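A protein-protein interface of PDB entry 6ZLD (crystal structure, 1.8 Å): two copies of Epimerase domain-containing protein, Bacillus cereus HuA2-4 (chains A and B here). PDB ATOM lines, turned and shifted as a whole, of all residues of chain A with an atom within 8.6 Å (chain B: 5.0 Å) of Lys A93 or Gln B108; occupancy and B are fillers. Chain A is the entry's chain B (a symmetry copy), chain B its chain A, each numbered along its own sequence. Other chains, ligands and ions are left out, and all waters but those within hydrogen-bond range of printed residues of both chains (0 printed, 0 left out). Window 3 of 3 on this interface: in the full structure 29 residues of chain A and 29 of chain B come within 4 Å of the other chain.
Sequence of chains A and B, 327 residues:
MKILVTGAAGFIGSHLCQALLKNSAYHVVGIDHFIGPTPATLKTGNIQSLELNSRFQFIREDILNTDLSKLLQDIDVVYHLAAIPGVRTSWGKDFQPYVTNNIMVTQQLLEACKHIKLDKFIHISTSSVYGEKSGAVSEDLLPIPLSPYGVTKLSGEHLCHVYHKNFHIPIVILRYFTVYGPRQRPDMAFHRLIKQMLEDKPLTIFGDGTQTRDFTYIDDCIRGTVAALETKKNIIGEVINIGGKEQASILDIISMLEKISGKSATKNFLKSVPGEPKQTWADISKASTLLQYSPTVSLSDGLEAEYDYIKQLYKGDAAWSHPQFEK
Of the 10 printed residues of chain A, 4 touch a printed residue of chain B. Of the 11 printed residues of chain B, 4 touch a printed residue of chain A. Hydrophobic or aromatic side chains of chain B within 4 Å of the printed part of chain A: Met B104. Among the printed residues, 7 pairs touch across the chains.
OE2 of Glu B111 is in hydrogen-bond range of N of Gly A92 (2.8 Å). O of Gly A92 sits close to OE1 of Gln B107 (3.0 Å).
Among the printed residues, merely in contact across the chains: Phe A95 with Gln B107, Phe A95 with Met B104, Lys A93 with Gln B108, Trp A91 with Glu B111 and Gly A92 with Gln B108.
Lys A93 touches one residue of chain B. Gln B108 touches just these residues of chain A: Gly A92 (3.8 Å) and Lys A93 (3.7 Å). Of chain A, only Gly A92 and Phe A95 come within 4 Å of Gln B107. Printed residues of chain A within 4 Å of Met B104: Phe A95 (3.6 Å). Printed residues of chain B within 4 Å of Gly A92: Gln B107, Gln B108 and Glu B111. Of the printed residues of chain A, Glu B111 touches Trp A91 (3.8 Å) and Gly A92 (2.8 Å). Printed residues of chain B within 4 Å of Phe A95: Met B104 and Gln B107. Printed residues of chain B within 4 Å of Trp A91: Glu B111 (3.8 Å). Leu B109 touches none of the printed residues of chain A.
No position is printed for both chains. Of the 7 pairs that touch across the chains among the printed residues, none has its exchanged pair printed and touching as well.
NE2 of Gln B107 is in hydrogen-bond range of OE1 of Gln B108.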
ATOM      1  N   THR A  89      -1.599 -14.249  -3.706  1.00  0.00           N
ATOM      2  CA  THR A  89      -0.721 -15.209  -4.418  1.00  0.00           C
ATOM      3  C   THR A  89      -1.567 -16.278  -5.119  1.00  0.00           C
ATOM      4  O   THR A  89      -1.089 -17.435  -5.195  1.00  0.00           O
ATOM      5  CB  THR A  89       0.286 -15.846  -3.448  1.00  0.00           C
ATOM      6  OG1 THR A  89      -0.438 -16.448  -2.362  1.00  0.00           O
ATOM      7  CG2 THR A  89       1.285 -14.851  -2.895  1.00  0.00           C
ATOM      8  N   SER A  90      -2.775 -15.926  -5.584  1.00  0.00           N
ATOM      9  CA  SER A  90      -3.737 -16.922  -6.134  1.00  0.00           C
ATOM     10  C   SER A  90      -3.896 -16.791  -7.655  1.00  0.00           C
ATOM     11  O   SER A  90      -4.878 -17.353  -8.170  1.00  0.00           O
ATOM     12  CB  SER A  90      -5.075 -16.868  -5.426  1.00  0.00           C
ATOM     13  OG  SER A  90      -5.775 -15.639  -5.581  1.00  0.00           O
ATOM     14  N   TRP A  91      -2.986 -16.096  -8.347  1.00  0.00           N
ATOM     15  CA  TRP A  91      -3.060 -15.813  -9.814  1.00  0.00           C
ATOM     16  C   TRP A  91      -2.279 -16.837 -10.628  1.00  0.00           C
ATOM     17  O   TRP A  91      -1.312 -17.453 -10.118  1.00  0.00           O
ATOM     18  CB  TRP A  91      -2.560 -14.396 -10.151  1.00  0.00           C
ATOM     19  CG  TRP A  91      -3.295 -13.319  -9.426  1.00  0.00           C
ATOM     20  CD1 TRP A  91      -2.861 -12.634  -8.330  1.00  0.00           C
ATOM     21  CD2 TRP A  91      -4.616 -12.830  -9.708  1.00  0.00           C
ATOM     22  NE1 TRP A  91      -3.808 -11.731  -7.925  1.00  0.00           N
ATOM     23  CE2 TRP A  91      -4.900 -11.838  -8.747  1.00  0.00           C
ATOM     24  CE3 TRP A  91      -5.566 -13.092 -10.703  1.00  0.00           C
ATOM     25  CZ2 TRP A  91      -6.090 -11.120  -8.762  1.00  0.00           C
ATOM     26  CZ3 TRP A  91      -6.742 -12.387 -10.701  1.00  0.00           C
ATOM     27  CH2 TRP A  91      -7.006 -11.421  -9.735  1.00  0.00           C
ATOM     28  N   GLY A  92      -2.641 -16.976 -11.909  1.00  0.00           N
ATOM     29  CA  GLY A  92      -1.816 -17.722 -12.871  1.00  0.00           C
ATOM     30  C   GLY A  92      -1.601 -19.164 -12.454  1.00  0.00           C
ATOM     31  O   GLY A  92      -2.579 -19.819 -12.069  1.00  0.00           O
ATOM     32  N   LYS A  93      -0.363 -19.656 -12.500  1.00  0.00           N
ATOM     33  CA  LYS A  93      -0.046 -21.068 -12.151  1.00  0.00           C
ATOM     34  C   LYS A  93      -0.158 -21.338 -10.639  1.00  0.00           C
ATOM     35  O   LYS A  93      -0.136 -22.513 -10.266  1.00  0.00           O
ATOM     36  CB  LYS A  93       1.338 -21.460 -12.677  1.00  0.00           C
ATOM     37  CG  LYS A  93       1.438 -21.611 -14.198  1.00  0.00           C
ATOM     38  CD  LYS A  93       0.254 -22.310 -14.863  1.00  0.00           C
ATOM     39  CE  LYS A  93       0.659 -23.457 -15.769  1.00  0.00           C
ATOM     40  NZ  LYS A  93      -0.507 -24.263 -16.197  1.00  0.00           N
ATOM     41  N   ASP A  94      -0.325 -20.321  -9.807  1.00  0.00           N
ATOM     42  CA  ASP A  94      -0.461 -20.475  -8.340  1.00  0.00           C
ATOM     43  C   ASP A  94      -1.898 -20.880  -7.982  1.00  0.00           C
ATOM     44  O   ASP A  94      -2.153 -21.173  -6.779  1.00  0.00           O
ATOM     45  CB  ASP A  94      -0.091 -19.172  -7.633  1.00  0.00           C
ATOM     46  CG  ASP A  94       1.377 -18.797  -7.771  1.00  0.00           C
ATOM     47  OD1 ASP A  94       2.204 -19.692  -7.869  1.00  0.00           O
ATOM     48  OD2 ASP A  94       1.658 -17.617  -7.767  1.00  0.00           O
ATOM     49  N   PHE A  95      -2.822 -20.837  -8.948  1.00  0.00           N
ATOM     50  CA  PHE A  95      -4.277 -20.989  -8.673  1.00  0.00           C
ATOM     51  C   PHE A  95      -4.576 -22.449  -8.304  1.00  0.00           C
ATOM     52  O   PHE A  95      -5.389 -22.696  -7.390  1.00  0.00           O
ATOM     53  CB  PHE A  95      -5.111 -20.504  -9.856  1.00  0.00           C
ATOM     54  CG  PHE A  95      -6.606 -20.652  -9.682  1.00  0.00           C
ATOM     55  CD1 PHE A  95      -7.298 -19.907  -8.733  1.00  0.00           C
ATOM     56  CD2 PHE A  95      -7.331 -21.449 -10.541  1.00  0.00           C
ATOM     57  CE1 PHE A  95      -8.679 -20.003  -8.613  1.00  0.00           C
ATOM     58  CE2 PHE A  95      -8.714 -21.518 -10.441  1.00  0.00           C
ATOM     59  CZ  PHE A  95      -9.380 -20.815  -9.468  1.00  0.00           C
ATOM     60  N   GLN A  96      -3.953 -23.395  -8.991  1.00  0.00           N
ATOM     61  CA  GLN A  96      -4.345 -24.835  -8.906  1.00  0.00           C
ATOM     62  C   GLN A  96      -4.344 -25.298  -7.446  1.00  0.00           C
ATOM     63  O   GLN A  96      -5.284 -25.934  -7.034  1.00  0.00           O
ATOM     64  CB  GLN A  96      -3.455 -25.710  -9.804  1.00  0.00           C
ATOM     65  CG  GLN A  96      -3.630 -27.214  -9.578  1.00  0.00           C
ATOM     66  CD  GLN A  96      -3.502 -28.091 -10.809  1.00  0.00           C
ATOM     67  OE1 GLN A  96      -3.581 -27.644 -11.951  1.00  0.00           O
ATOM     68  NE2 GLN A  96      -3.359 -29.389 -10.584  1.00  0.00           N
ATOM     69  N   PRO A  97      -3.294 -25.078  -6.619  1.00  0.00           N
ATOM     70  CA  PRO A  97      -3.337 -25.488  -5.202  1.00  0.00           C
ATOM     71  C   PRO A  97      -4.533 -24.967  -4.387  1.00  0.00           C
ATOM     72  O   PRO A  97      -5.005 -25.664  -3.493  1.00  0.00           O
ATOM     73  CB  PRO A  97      -2.031 -24.921  -4.640  1.00  0.00           C
ATOM     74  CG  PRO A  97      -1.121 -24.943  -5.850  1.00  0.00           C
ATOM     75  CD  PRO A  97      -1.998 -24.506  -7.000  1.00  0.00           C
ATOM     76  N   TYR A  98      -5.033 -23.786  -4.717  1.00  0.00           N
ATOM     77  CA  TYR A  98      -6.264 -23.218  -4.102  1.00  0.00           C
ATOM     78  C   TYR A  98      -7.477 -24.070  -4.504  1.00  0.00           C
ATOM     79  O   TYR A  98      -8.280 -24.380  -3.656  1.00  0.00           O
ATOM     80  CB  TYR A  98      -6.493 -21.763  -4.505  1.00  0.00           C
ATOM     81  CG  TYR A  98      -5.517 -20.774  -3.926  1.00  0.00           C
ATOM     82  CD1 TYR A  98      -4.267 -20.567  -4.495  1.00  0.00           C
ATOM     83  CD2 TYR A  98      -5.863 -19.991  -2.833  1.00  0.00           C
ATOM     84  CE1 TYR A  98      -3.378 -19.639  -3.969  1.00  0.00           C
ATOM     85  CE2 TYR A  98      -4.985 -19.063  -2.303  1.00  0.00           C
ATOM     86  CZ  TYR A  98      -3.739 -18.876  -2.874  1.00  0.00           C
ATOM     87  OH  TYR A  98      -2.888 -17.942  -2.334  1.00  0.00           O
ATOM     88  N   LEU B  64      -6.785 -27.097 -21.464  1.00  0.00           N
ATOM     89  CA  LEU B  64      -5.776 -27.106 -20.380  1.00  0.00           C
ATOM     90  C   LEU B  64      -4.390 -27.549 -20.906  1.00  0.00           C
ATOM     91  O   LEU B  64      -3.403 -27.332 -20.192  1.00  0.00           O
ATOM     92  CB  LEU B  64      -6.246 -28.032 -19.254  1.00  0.00           C
ATOM     93  CG  LEU B  64      -7.352 -27.458 -18.380  1.00  0.00           C
ATOM     94  CD1 LEU B  64      -7.700 -28.406 -17.269  1.00  0.00           C
ATOM     95  CD2 LEU B  64      -6.954 -26.122 -17.804  1.00  0.00           C
ATOM     96  N   LEU B  68      -2.315 -21.472 -25.422  1.00  0.00           N
ATOM     97  CA  LEU B  68      -3.456 -20.521 -25.366  1.00  0.00           C
ATOM     98  C   LEU B  68      -3.020 -19.200 -26.011  1.00  0.00           C
ATOM     99  O   LEU B  68      -3.871 -18.530 -26.569  1.00  0.00           O
ATOM    100  CB  LEU B  68      -3.939 -20.359 -23.923  1.00  0.00           C
ATOM    101  CG  LEU B  68      -4.697 -21.561 -23.361  1.00  0.00           C
ATOM    102  CD1 LEU B  68      -4.994 -21.384 -21.869  1.00  0.00           C
ATOM    103  CD2 LEU B  68      -5.984 -21.787 -24.129  1.00  0.00           C
ATOM    104  N   MET B 104     -10.882 -24.716 -13.591  1.00  0.00           N
ATOM    105  CA  MET B 104      -9.475 -24.512 -14.044  1.00  0.00           C
ATOM    106  C   MET B 104      -9.473 -23.996 -15.497  1.00  0.00           C
ATOM    107  O   MET B 104      -8.688 -23.085 -15.804  1.00  0.00           O
ATOM    108  CB  MET B 104      -8.621 -25.782 -13.935  1.00  0.00           C
ATOM    109  CG  MET B 104      -8.334 -26.196 -12.494  1.00  0.00           C
ATOM    110  SD  MET B 104      -7.483 -24.890 -11.617  1.00  0.00           S
ATOM    111  CE  MET B 104      -6.096 -24.581 -12.711  1.00  0.00           C
ATOM    112  N   VAL B 105     -10.284 -24.569 -16.382  1.00  0.00           N
ATOM    113  CA  VAL B 105     -10.354 -24.142 -17.808  1.00  0.00           C
ATOM    114  C   VAL B 105     -10.733 -22.664 -17.878  1.00  0.00           C
ATOM    115  O   VAL B 105     -10.102 -21.939 -18.656  1.00  0.00           O
ATOM    116  CB  VAL B 105     -11.334 -25.005 -18.616  1.00  0.00           C
ATOM    117  CG1 VAL B 105     -11.800 -24.333 -19.893  1.00  0.00           C
ATOM    118  CG2 VAL B 105     -10.728 -26.344 -18.930  1.00  0.00           C
ATOM    119  N   THR B 106     -11.750 -22.230 -17.133  1.00  0.00           N
ATOM    120  CA  THR B 106     -12.207 -20.819 -17.205  1.00  0.00           C
ATOM    121  C   THR B 106     -11.054 -19.919 -16.769  1.00  0.00           C
ATOM    122  O   THR B 106     -10.763 -18.919 -17.448  1.00  0.00           O
ATOM    123  CB  THR B 106     -13.450 -20.642 -16.341  1.00  0.00           C
ATOM    124  OG1 THR B 106     -14.442 -21.532 -16.855  1.00  0.00           O
ATOM    125  CG2 THR B 106     -13.948 -19.217 -16.311  1.00  0.00           C
ATOM    126  N   GLN B 107     -10.427 -20.244 -15.634  1.00  0.00           N
ATOM    127  CA  GLN B 107      -9.295 -19.454 -15.103  1.00  0.00           C
ATOM    128  C   GLN B 107      -8.168 -19.380 -16.135  1.00  0.00           C
ATOM    129  O   GLN B 107      -7.582 -18.306 -16.270  1.00  0.00           O
ATOM    130  CB  GLN B 107      -8.772 -20.005 -13.786  1.00  0.00           C
ATOM    131  CG  GLN B 107      -7.700 -19.100 -13.174  1.00  0.00           C
ATOM    132  CD  GLN B 107      -6.283 -19.595 -13.345  1.00  0.00           C
ATOM    133  OE1 GLN B 107      -5.321 -19.010 -12.815  1.00  0.00           O
ATOM    134  NE2 GLN B 107      -6.135 -20.702 -14.043  1.00  0.00           N
ATOM    135  N   GLN B 108      -7.807 -20.480 -16.764  1.00  0.00           N
ATOM    136  CA  GLN B 108      -6.647 -20.482 -17.688  1.00  0.00           C
ATOM    137  C   GLN B 108      -6.982 -19.653 -18.942  1.00  0.00           C
ATOM    138  O   GLN B 108      -6.069 -18.923 -19.429  1.00  0.00           O
ATOM    139  CB  GLN B 108      -6.199 -21.911 -17.945  1.00  0.00           C
ATOM    140  CG  GLN B 108      -5.667 -22.588 -16.674  1.00  0.00           C
ATOM    141  CD  GLN B 108      -4.315 -22.083 -16.219  1.00  0.00           C
ATOM    142  OE1 GLN B 108      -4.126 -21.636 -15.074  1.00  0.00           O
ATOM    143  NE2 GLN B 108      -3.356 -22.155 -17.130  1.00  0.00           N
ATOM    144  N   LEU B 109      -8.221 -19.712 -19.423  1.00  0.00           N
ATOM    145  CA  LEU B 109      -8.671 -18.863 -20.553  1.00  0.00           C
ATOM    146  C   LEU B 109      -8.575 -17.398 -20.135  1.00  0.00           C
ATOM    147  O   LEU B 109      -8.092 -16.603 -20.951  1.00  0.00           O
ATOM    148  CB  LEU B 109     -10.107 -19.204 -20.955  1.00  0.00           C
ATOM    149  CG  LEU B 109     -10.258 -20.366 -21.929  1.00  0.00           C
ATOM    150  CD1 LEU B 109     -11.723 -20.747 -22.082  1.00  0.00           C
ATOM    151  CD2 LEU B 109      -9.638 -20.039 -23.297  1.00  0.00           C
ATOM    152  N   LEU B 110      -9.078 -17.045 -18.949  1.00  0.00           N
ATOM    153  CA  LEU B 110      -9.138 -15.633 -18.501  1.00  0.00           C
ATOM    154  C   LEU B 110      -7.719 -15.086 -18.323  1.00  0.00           C
ATOM    155  O   LEU B 110      -7.510 -13.888 -18.677  1.00  0.00           O
ATOM    156  CB  LEU B 110      -9.954 -15.537 -17.214  1.00  0.00           C
ATOM    157  CG  LEU B 110     -11.454 -15.748 -17.394  1.00  0.00           C
ATOM    158  CD1 LEU B 110     -12.161 -15.848 -16.042  1.00  0.00           C
ATOM    159  CD2 LEU B 110     -12.037 -14.624 -18.240  1.00  0.00           C
ATOM    160  N   GLU B 111      -6.790 -15.917 -17.835  1.00  0.00           N
ATOM    161  CA  GLU B 111      -5.364 -15.546 -17.680  1.00  0.00           C
ATOM    162  C   GLU B 111      -4.822 -15.227 -19.079  1.00  0.00           C
ATOM    163  O   GLU B 111      -4.210 -14.151 -19.239  1.00  0.00           O
ATOM    164  CB  GLU B 111      -4.575 -16.657 -16.966  1.00  0.00           C
ATOM    165  CG  GLU B 111      -4.763 -16.680 -15.453  1.00  0.00           C
ATOM    166  CD  GLU B 111      -3.962 -15.653 -14.679  1.00  0.00           C
ATOM    167  OE1 GLU B 111      -3.031 -15.112 -15.246  1.00  0.00           O
ATOM    168  OE2 GLU B 111      -4.263 -15.403 -13.516  1.00  0.00           O
ATOM    169  N   ALA B 112      -5.071 -16.098 -20.059  1.00  0.00           N
ATOM    170  CA  ALA B 112      -4.581 -15.937 -21.455  1.00  0.00           C
ATOM    171  C   ALA B 112      -5.134 -14.648 -22.087  1.00  0.00           C
ATOM    172  O   ALA B 112      -4.418 -14.046 -22.907  1.00  0.00           O
ATOM    173  CB  ALA B 112      -4.864 -17.167 -22.280  1.00  0.00           C
